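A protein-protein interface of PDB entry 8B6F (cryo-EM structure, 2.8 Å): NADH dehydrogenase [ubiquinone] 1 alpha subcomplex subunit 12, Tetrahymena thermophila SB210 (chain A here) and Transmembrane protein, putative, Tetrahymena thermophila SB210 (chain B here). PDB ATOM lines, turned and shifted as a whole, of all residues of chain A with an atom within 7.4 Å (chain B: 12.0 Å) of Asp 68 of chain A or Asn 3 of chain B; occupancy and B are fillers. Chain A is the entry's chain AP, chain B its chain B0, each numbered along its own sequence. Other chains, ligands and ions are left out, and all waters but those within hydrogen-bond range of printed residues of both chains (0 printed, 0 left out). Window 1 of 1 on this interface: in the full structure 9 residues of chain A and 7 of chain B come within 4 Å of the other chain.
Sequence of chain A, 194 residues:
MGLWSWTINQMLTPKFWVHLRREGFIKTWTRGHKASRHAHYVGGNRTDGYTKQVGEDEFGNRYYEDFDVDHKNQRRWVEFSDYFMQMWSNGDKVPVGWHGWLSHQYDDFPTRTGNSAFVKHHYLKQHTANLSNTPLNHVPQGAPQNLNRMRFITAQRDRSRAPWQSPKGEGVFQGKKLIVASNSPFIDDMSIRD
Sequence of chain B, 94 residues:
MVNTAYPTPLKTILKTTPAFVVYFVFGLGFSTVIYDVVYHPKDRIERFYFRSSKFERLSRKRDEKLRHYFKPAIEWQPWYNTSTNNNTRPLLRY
Asn 3 of chain B touches three residues of chain A. No residue of chain B comes within 4 Å of Asn 45 of chain A. Of chain B, only Val 2 (3.9 Å), Asn 3 (3.2 Å), Thr 4 (3.1 Å) and Ala 5 (3.96 Å) come within 4 Å of Thr 47 of chain A. Asp 48 of chain A touches just one residue of chain B: Val 2 (3.8 Å). No residue of chain B comes within 4 Å of Phe 67 of chain A. No residue of chain B comes within 4 Å of Val 69 of chain A. Printed residues of chain A within 4 Å of Lys 11 of chain B: Tyr 41 and Asp 70. Printed residues of chain A within 4 Å of Thr 4 of chain B: Thr 47 (3.1 Å). Of the printed residues of chain B, Tyr 41 of chain A touches Lys 11. Of the printed residues of chain A, Ala 5 of chain B touches Thr 47. Thr 51 of chain A touches none of the printed residues of chain B.
Among the printed residues, 9 pairs touch across the chains.
The side-chain amide oxygen (OD1) of Asn 3 of chain B sits close to the backbone NH (N) of Ala 5 of chain B, 3.5 Å away. The guanidinium group (NE) of Arg 46 of chain A is in salt-bridge range of the side-chain carboxylate (OD1) of Asp 48 of chain A, at 3.5 Å. The side-chain hydroxyl (OH) of Tyr 41 of chain A lies close to the side-chain amide oxygen (OE1) of Gln 74 of chain A (3.2 Å). The side-chain hydroxyl (OH) of Tyr 41 of chain A is in hydrogen-bond range of the backbone NH (N) of Asp 70 of chain A. ND2 of Asn 45 of chain A lies within hydrogen-bond range of O of Asp 68 of chain A (2.5 Å). NH1 of Arg 46 of chain A lies within salt-bridge range of OD2 of Asp 68 of chain A, at 2.6 Å.
Among the printed residues, pairs that only touch across the chains: Arg 46 of chain A with Asn 3 of chain B (3.4 Å), Asp 48 of chain A with Val 2 of chain B (3.8 Å), Asp 68 of chain A with Asn 3 of chain B (3.9 Å), Thr 47 of chain A with Val 2 of chain B (3.9 Å) and Thr 47 of chain A with Ala 5 of chain B (3.96 Å).
The side-chain amide oxygen (OD1) of Asn 3 of chain B lies within hydrogen-bond range of the backbone NH (N) of Thr 47 of chain A, at 3.2 Å. The side-chain carboxylate (OD1) of Asp 70 of chain A lies within salt-bridge range of the side-chain amino group (NZ) of Lys 11 of chain B (3.9 Å). The backbone NH (N) of Thr 4 of chain B sits at hydrogen-bond distance from the side-chain hydroxyl (OG1) of Thr 47 of chain A (3.1 Å). NZ of Lys 11 of chain B sits close to OH of Tyr 41 of chain A (3.4 Å).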
ATOM      1  N   TYR A  41      14.425   9.869 -16.722  1.00  0.00           N
ATOM      2  CA  TYR A  41      13.650  10.092 -15.510  1.00  0.00           C
ATOM      3  C   TYR A  41      12.377   9.261 -15.453  1.00  0.00           C
ATOM      4  O   TYR A  41      11.614   9.392 -14.491  1.00  0.00           O
ATOM      5  CB  TYR A  41      13.280  11.574 -15.379  1.00  0.00           C
ATOM      6  CG  TYR A  41      14.427  12.504 -15.038  1.00  0.00           C
ATOM      7  CD1 TYR A  41      15.686  12.015 -14.711  1.00  0.00           C
ATOM      8  CD2 TYR A  41      14.238  13.879 -15.030  1.00  0.00           C
ATOM      9  CE1 TYR A  41      16.721  12.870 -14.395  1.00  0.00           C
ATOM     10  CE2 TYR A  41      15.266  14.740 -14.717  1.00  0.00           C
ATOM     11  CZ  TYR A  41      16.505  14.232 -14.400  1.00  0.00           C
ATOM     12  OH  TYR A  41      17.530  15.093 -14.086  1.00  0.00           O
ATOM     13  N   GLY A  44      11.942   7.505 -12.230  1.00  0.00           N
ATOM     14  CA  GLY A  44      12.998   7.948 -11.347  1.00  0.00           C
ATOM     15  C   GLY A  44      14.356   7.919 -12.031  1.00  0.00           C
ATOM     16  O   GLY A  44      14.578   7.218 -13.022  1.00  0.00           O
ATOM     17  N   ASN A  45      15.283   8.703 -11.477  1.00  0.00           N
ATOM     18  CA  ASN A  45      16.607   8.818 -12.078  1.00  0.00           C
ATOM     19  C   ASN A  45      17.471   7.595 -11.789  1.00  0.00           C
ATOM     20  O   ASN A  45      18.252   7.170 -12.647  1.00  0.00           O
ATOM     21  CB  ASN A  45      17.295  10.085 -11.575  1.00  0.00           C
ATOM     22  CG  ASN A  45      18.554  10.409 -12.350  1.00  0.00           C
ATOM     23  OD1 ASN A  45      18.749   9.935 -13.468  1.00  0.00           O
ATOM     24  ND2 ASN A  45      19.418  11.225 -11.759  1.00  0.00           N
ATOM     25  N   ARG A  46      17.355   7.024 -10.595  1.00  0.00           N
ATOM     26  CA  ARG A  46      18.151   5.858 -10.242  1.00  0.00           C
ATOM     27  C   ARG A  46      17.736   4.651 -11.077  1.00  0.00           C
ATOM     28  O   ARG A  46      16.584   4.525 -11.496  1.00  0.00           O
ATOM     29  CB  ARG A  46      18.005   5.551  -8.754  1.00  0.00           C
ATOM     30  CG  ARG A  46      18.489   6.679  -7.857  1.00  0.00           C
ATOM     31  CD  ARG A  46      18.361   6.310  -6.396  1.00  0.00           C
ATOM     32  NE  ARG A  46      19.227   5.194  -6.030  1.00  0.00           N
ATOM     33  CZ  ARG A  46      20.490   5.307  -5.647  1.00  0.00           C
ATOM     34  NH1 ARG A  46      21.089   6.483  -5.573  1.00  0.00           N
ATOM     35  NH2 ARG A  46      21.170   4.209  -5.331  1.00  0.00           N
ATOM     36  N   THR A  47      18.695   3.756 -11.312  1.00  0.00           N
ATOM     37  CA  THR A  47      18.478   2.592 -12.164  1.00  0.00           C
ATOM     38  C   THR A  47      18.177   1.317 -11.393  1.00  0.00           C
ATOM     39  O   THR A  47      17.507   0.428 -11.929  1.00  0.00           O
ATOM     40  CB  THR A  47      19.704   2.347 -13.050  1.00  0.00           C
ATOM     41  OG1 THR A  47      20.837   2.035 -12.229  1.00  0.00           O
ATOM     42  CG2 THR A  47      20.011   3.576 -13.890  1.00  0.00           C
ATOM     43  N   ASP A  48      18.656   1.198 -10.155  1.00  0.00           N
ATOM     44  CA  ASP A  48      18.438  -0.016  -9.376  1.00  0.00           C
ATOM     45  C   ASP A  48      17.004  -0.155  -8.883  1.00  0.00           C
ATOM     46  O   ASP A  48      16.641  -1.227  -8.389  1.00  0.00           O
ATOM     47  CB  ASP A  48      19.399  -0.055  -8.185  1.00  0.00           C
ATOM     48  CG  ASP A  48      19.348   1.210  -7.355  1.00  0.00           C
ATOM     49  OD1 ASP A  48      19.053   2.280  -7.925  1.00  0.00           O
ATOM     50  OD2 ASP A  48      19.610   1.136  -6.136  1.00  0.00           O
ATOM     51  N   GLY A  49      16.190   0.887  -8.999  1.00  0.00           N
ATOM     52  CA  GLY A  49      14.805   0.815  -8.571  1.00  0.00           C
ATOM     53  C   GLY A  49      14.079   2.078  -8.966  1.00  0.00           C
ATOM     54  O   GLY A  49      14.688   3.064  -9.387  1.00  0.00           O
ATOM     55  N   THR A  51      11.243   5.180  -8.037  1.00  0.00           N
ATOM     56  CA  THR A  51      10.860   5.992  -6.892  1.00  0.00           C
ATOM     57  C   THR A  51       9.537   5.515  -6.313  1.00  0.00           C
ATOM     58  O   THR A  51       8.594   5.205  -7.044  1.00  0.00           O
ATOM     59  CB  THR A  51      10.745   7.461  -7.304  1.00  0.00           C
ATOM     60  OG1 THR A  51      11.969   7.889  -7.913  1.00  0.00           O
ATOM     61  CG2 THR A  51      10.457   8.340  -6.098  1.00  0.00           C
ATOM     62  N   GLU A  65       8.694  11.874  -5.550  1.00  0.00           N
ATOM     63  CA  GLU A  65       9.797  12.737  -5.141  1.00  0.00           C
ATOM     64  C   GLU A  65      11.087  11.937  -5.213  1.00  0.00           C
ATOM     65  O   GLU A  65      11.214  10.906  -4.547  1.00  0.00           O
ATOM     66  CB  GLU A  65       9.581  13.286  -3.729  1.00  0.00           C
ATOM     67  CG  GLU A  65      10.681  14.227  -3.267  1.00  0.00           C
ATOM     68  CD  GLU A  65      10.397  14.832  -1.909  1.00  0.00           C
ATOM     69  OE1 GLU A  65       9.423  14.398  -1.259  1.00  0.00           O
ATOM     70  OE2 GLU A  65      11.143  15.741  -1.492  1.00  0.00           O
ATOM     71  N   ASP A  66      12.039  12.412  -6.017  1.00  0.00           N
ATOM     72  CA  ASP A  66      13.336  11.769  -6.174  1.00  0.00           C
ATOM     73  C   ASP A  66      14.430  12.782  -5.881  1.00  0.00           C
ATOM     74  O   ASP A  66      14.405  13.895  -6.414  1.00  0.00           O
ATOM     75  CB  ASP A  66      13.501  11.203  -7.589  1.00  0.00           C
ATOM     76  CG  ASP A  66      14.807  10.452  -7.771  1.00  0.00           C
ATOM     77  OD1 ASP A  66      15.577  10.343  -6.795  1.00  0.00           O
ATOM     78  OD2 ASP A  66      15.064   9.969  -8.893  1.00  0.00           O
ATOM     79  N   PHE A  67      15.388  12.395  -5.043  1.00  0.00           N
ATOM     80  CA  PHE A  67      16.479  13.276  -4.647  1.00  0.00           C
ATOM     81  C   PHE A  67      17.732  13.103  -5.495  1.00  0.00           C
ATOM     82  O   PHE A  67      18.730  13.783  -5.237  1.00  0.00           O
ATOM     83  CB  PHE A  67      16.829  13.044  -3.173  1.00  0.00           C
ATOM     84  CG  PHE A  67      15.815  13.598  -2.217  1.00  0.00           C
ATOM     85  CD1 PHE A  67      14.700  12.858  -1.862  1.00  0.00           C
ATOM     86  CD2 PHE A  67      15.977  14.861  -1.673  1.00  0.00           C
ATOM     87  CE1 PHE A  67      13.766  13.367  -0.983  1.00  0.00           C
ATOM     88  CE2 PHE A  67      15.048  15.375  -0.793  1.00  0.00           C
ATOM     89  CZ  PHE A  67      13.940  14.627  -0.448  1.00  0.00           C
ATOM     90  N   ASP A  68      17.716  12.217  -6.490  1.00  0.00           N
ATOM     91  CA  ASP A  68      18.864  12.002  -7.360  1.00  0.00           C
ATOM     92  C   ASP A  68      18.728  12.711  -8.700  1.00  0.00           C
ATOM     93  O   ASP A  68      19.547  12.483  -9.595  1.00  0.00           O
ATOM     94  CB  ASP A  68      19.087  10.505  -7.584  1.00  0.00           C
ATOM     95  CG  ASP A  68      19.759   9.835  -6.405  1.00  0.00           C
ATOM     96  OD1 ASP A  68      19.887  10.482  -5.345  1.00  0.00           O
ATOM     97  OD2 ASP A  68      20.178   8.668  -6.543  1.00  0.00           O
ATOM     98  N   VAL A  69      17.715  13.563  -8.863  1.00  0.00           N
ATOM     99  CA  VAL A  69      17.595  14.330 -10.093  1.00  0.00           C
ATOM    100  C   VAL A  69      18.807  15.244 -10.238  1.00  0.00           C
ATOM    101  O   VAL A  69      19.399  15.696  -9.251  1.00  0.00           O
ATOM    102  CB  VAL A  69      16.287  15.139 -10.118  1.00  0.00           C
ATOM    103  CG1 VAL A  69      15.094  14.209 -10.230  1.00  0.00           C
ATOM    104  CG2 VAL A  69      16.169  16.011  -8.876  1.00  0.00           C
ATOM    105  N   ASP A  70      19.185  15.513 -11.488  1.00  0.00           N
ATOM    106  CA  ASP A  70      20.385  16.294 -11.757  1.00  0.00           C
ATOM    107  C   ASP A  70      20.221  17.773 -11.435  1.00  0.00           C
ATOM    108  O   ASP A  70      21.227  18.489 -11.398  1.00  0.00           O
ATOM    109  CB  ASP A  70      20.794  16.136 -13.220  1.00  0.00           C
ATOM    110  CG  ASP A  70      21.118  14.702 -13.581  1.00  0.00           C
ATOM    111  OD1 ASP A  70      21.537  13.941 -12.685  1.00  0.00           O
ATOM    112  OD2 ASP A  70      20.954  14.335 -14.761  1.00  0.00           O
ATOM    113  N   HIS A  71      18.999  18.247 -11.207  1.00  0.00           N
ATOM    114  CA  HIS A  71      18.760  19.643 -10.877  1.00  0.00           C
ATOM    115  C   HIS A  71      17.854  19.733  -9.659  1.00  0.00           C
ATOM    116  O   HIS A  71      16.995  18.877  -9.435  1.00  0.00           O
ATOM    117  CB  HIS A  71      18.137  20.402 -12.050  1.00  0.00           C
ATOM    118  CG  HIS A  71      18.265  21.889 -11.936  1.00  0.00           C
ATOM    119  ND1 HIS A  71      17.190  22.713 -11.679  1.00  0.00           N
ATOM    120  CD2 HIS A  71      19.345  22.699 -12.034  1.00  0.00           C
ATOM    121  CE1 HIS A  71      17.604  23.967 -11.629  1.00  0.00           C
ATOM    122  NE2 HIS A  71      18.907  23.986 -11.840  1.00  0.00           N
ATOM    123  N   GLN A  74      13.721  19.743  -9.812  1.00  0.00           N
ATOM    124  CA  GLN A  74      13.047  18.614 -10.443  1.00  0.00           C
ATOM    125  C   GLN A  74      12.790  17.472  -9.463  1.00  0.00           C
ATOM    126  O   GLN A  74      12.487  16.357  -9.896  1.00  0.00           O
ATOM    127  CB  GLN A  74      13.866  18.103 -11.630  1.00  0.00           C
ATOM    128  CG  GLN A  74      14.099  19.143 -12.712  1.00  0.00           C
ATOM    129  CD  GLN A  74      15.044  18.654 -13.787  1.00  0.00           C
ATOM    130  OE1 GLN A  74      15.706  17.630 -13.629  1.00  0.00           O
ATOM    131  NE2 GLN A  74      15.111  19.386 -14.893  1.00  0.00           N
ATOM    132  N   ARG A  75      12.900  17.719  -8.156  1.00  0.00           N
ATOM    133  CA  ARG A  75      12.735  16.638  -7.186  1.00  0.00           C
ATOM    134  C   ARG A  75      11.330  16.052  -7.245  1.00  0.00           C
ATOM    135  O   ARG A  75      11.156  14.831  -7.311  1.00  0.00           O
ATOM    136  CB  ARG A  75      13.036  17.138  -5.773  1.00  0.00           C
ATOM    137  CG  ARG A  75      14.482  17.527  -5.533  1.00  0.00           C
ATOM    138  CD  ARG A  75      14.833  17.409  -4.059  1.00  0.00           C
ATOM    139  NE  ARG A  75      13.800  17.984  -3.204  1.00  0.00           N
ATOM    140  CZ  ARG A  75      13.754  19.253  -2.824  1.00  0.00           C
ATOM    141  NH1 ARG A  75      14.674  20.124  -3.204  1.00  0.00           N
ATOM    142  NH2 ARG A  75      12.760  19.659  -2.040  1.00  0.00           N
ATOM    143  N   VAL B   2      23.535   0.621  -5.985  1.00  0.00           N
ATOM    144  CA  VAL B   2      24.322   0.598  -7.248  1.00  0.00           C
ATOM    145  C   VAL B   2      23.553   1.296  -8.361  1.00  0.00           C
ATOM    146  O   VAL B   2      22.952   0.651  -9.218  1.00  0.00           O
ATOM    147  CB  VAL B   2      24.680  -0.844  -7.659  1.00  0.00           C
ATOM    148  CG1 VAL B   2      25.820  -1.367  -6.802  1.00  0.00           C
ATOM    149  CG2 VAL B   2      23.465  -1.760  -7.548  1.00  0.00           C
ATOM    150  N   ASN B   3      23.575   2.626  -8.340  1.00  0.00           N
ATOM    151  CA  ASN B   3      22.917   3.436  -9.361  1.00  0.00           C
ATOM    152  C   ASN B   3      23.873   3.582 -10.536  1.00  0.00           C
ATOM    153  O   ASN B   3      24.702   4.491 -10.587  1.00  0.00           O
ATOM    154  CB  ASN B   3      22.512   4.790  -8.793  1.00  0.00           C
ATOM    155  CG  ASN B   3      21.909   5.702  -9.839  1.00  0.00           C
ATOM    156  OD1 ASN B   3      21.446   5.246 -10.883  1.00  0.00           O
ATOM    157  ND2 ASN B   3      21.906   7.000  -9.561  1.00  0.00           N
ATOM    158  N   THR B   4      23.760   2.665 -11.496  1.00  0.00           N
ATOM    159  CA  THR B   4      24.616   2.674 -12.682  1.00  0.00           C
ATOM    160  C   THR B   4      24.018   3.573 -13.766  1.00  0.00           C
ATOM    161  O   THR B   4      23.746   3.156 -14.890  1.00  0.00           O
ATOM    162  CB  THR B   4      24.826   1.253 -13.194  1.00  0.00           C
ATOM    163  OG1 THR B   4      23.564   0.680 -13.563  1.00  0.00           O
ATOM    164  CG2 THR B   4      25.481   0.391 -12.125  1.00  0.00           C
ATOM    165  N   ALA B   5      23.813   4.833 -13.399  1.00  0.00           N
ATOM    166  CA  ALA B   5      23.257   5.807 -14.322  1.00  0.00           C
ATOM    167  C   ALA B   5      24.346   6.360 -15.238  1.00  0.00           C
ATOM    168  O   ALA B   5      25.546   6.201 -14.996  1.00  0.00           O
ATOM    169  CB  ALA B   5      22.581   6.941 -13.554  1.00  0.00           C
ATOM    170  N   TYR B   6      23.911   7.017 -16.309  1.00  0.00           N
ATOM    171  CA  TYR B   6      24.847   7.627 -17.236  1.00  0.00           C
ATOM    172  C   TYR B   6      25.578   8.788 -16.563  1.00  0.00           C
ATOM    173  O   TYR B   6      25.060   9.397 -15.624  1.00  0.00           O
ATOM    174  CB  TYR B   6      24.122   8.144 -18.474  1.00  0.00           C
ATOM    175  CG  TYR B   6      23.641   7.074 -19.425  1.00  0.00           C
ATOM    176  CD1 TYR B   6      22.589   6.236 -19.087  1.00  0.00           C
ATOM    177  CD2 TYR B   6      24.216   6.930 -20.678  1.00  0.00           C
ATOM    178  CE1 TYR B   6      22.139   5.267 -19.963  1.00  0.00           C
ATOM    179  CE2 TYR B   6      23.774   5.967 -21.560  1.00  0.00           C
ATOM    180  CZ  TYR B   6      22.735   5.138 -21.197  1.00  0.00           C
ATOM    181  OH  TYR B   6      22.291   4.178 -22.074  1.00  0.00           O
ATOM    182  N   PRO B   7      26.787   9.109 -17.017  1.00  0.00           N
ATOM    183  CA  PRO B   7      27.415  10.361 -16.586  1.00  0.00           C
ATOM    184  C   PRO B   7      26.573  11.559 -16.997  1.00  0.00           C
ATOM    185  O   PRO B   7      25.891  11.546 -18.023  1.00  0.00           O
ATOM    186  CB  PRO B   7      28.767  10.351 -17.309  1.00  0.00           C
ATOM    187  CG  PRO B   7      29.038   8.922 -17.586  1.00  0.00           C
ATOM    188  CD  PRO B   7      27.702   8.287 -17.826  1.00  0.00           C
ATOM    189  N   THR B   8      26.624  12.600 -16.173  1.00  0.00           N
ATOM    190  CA  THR B   8      25.840  13.802 -16.448  1.00  0.00           C
ATOM    191  C   THR B   8      26.139  14.401 -17.814  1.00  0.00           C
ATOM    192  O   THR B   8      25.186  14.705 -18.552  1.00  0.00           O
ATOM    193  CB  THR B   8      26.070  14.825 -15.333  1.00  0.00           C
ATOM    194  OG1 THR B   8      25.314  14.452 -14.174  1.00  0.00           O
ATOM    195  CG2 THR B   8      25.663  16.223 -15.780  1.00  0.00           C
ATOM    196  N   PRO B   9      27.396  14.615 -18.214  1.00  0.00           N
ATOM    197  CA  PRO B   9      27.629  15.193 -19.548  1.00  0.00           C
ATOM    198  C   PRO B   9      27.068  14.346 -20.672  1.00  0.00           C
ATOM    199  O   PRO B   9      26.461  14.886 -21.603  1.00  0.00           O
ATOM    200  CB  PRO B   9      29.161  15.301 -19.620  1.00  0.00           C
ATOM    201  CG  PRO B   9      29.670  14.376 -18.583  1.00  0.00           C
ATOM    202  CD  PRO B   9      28.656  14.390 -17.488  1.00  0.00           C
ATOM    203  N   LYS B  11      24.561  12.173 -20.524  1.00  0.00           N
ATOM    204  CA  LYS B  11      23.103  12.216 -20.481  1.00  0.00           C
ATOM    205  C   LYS B  11      22.573  13.516 -21.072  1.00  0.00           C
ATOM    206  O   LYS B  11      21.562  13.517 -21.784  1.00  0.00           O
ATOM    207  CB  LYS B  11      22.613  12.045 -19.044  1.00  0.00           C
ATOM    208  CG  LYS B  11      21.200  11.499 -18.953  1.00  0.00           C
ATOM    209  CD  LYS B  11      20.640  11.590 -17.546  1.00  0.00           C
ATOM    210  CE  LYS B  11      20.223  13.012 -17.214  1.00  0.00           C
ATOM    211  NZ  LYS B  11      19.532  13.091 -15.897  1.00  0.00           N
ATOM    212  N   THR B  12      23.234  14.634 -20.781  1.00  0.00           N
ATOM    213  CA  THR B  12      22.833  15.906 -21.373  1.00  0.00           C
ATOM    214  C   THR B  12      23.010  15.886 -22.888  1.00  0.00           C
ATOM    215  O   THR B  12      22.145  16.367 -23.627  1.00  0.00           O
ATOM    216  CB  THR B  12      23.643  17.046 -20.754  1.00  0.00           C
ATOM    217  OG1 THR B  12      23.402  17.096 -19.342  1.00  0.00           O
ATOM    218  CG2 THR B  12      23.267  18.385 -21.371  1.00  0.00           C
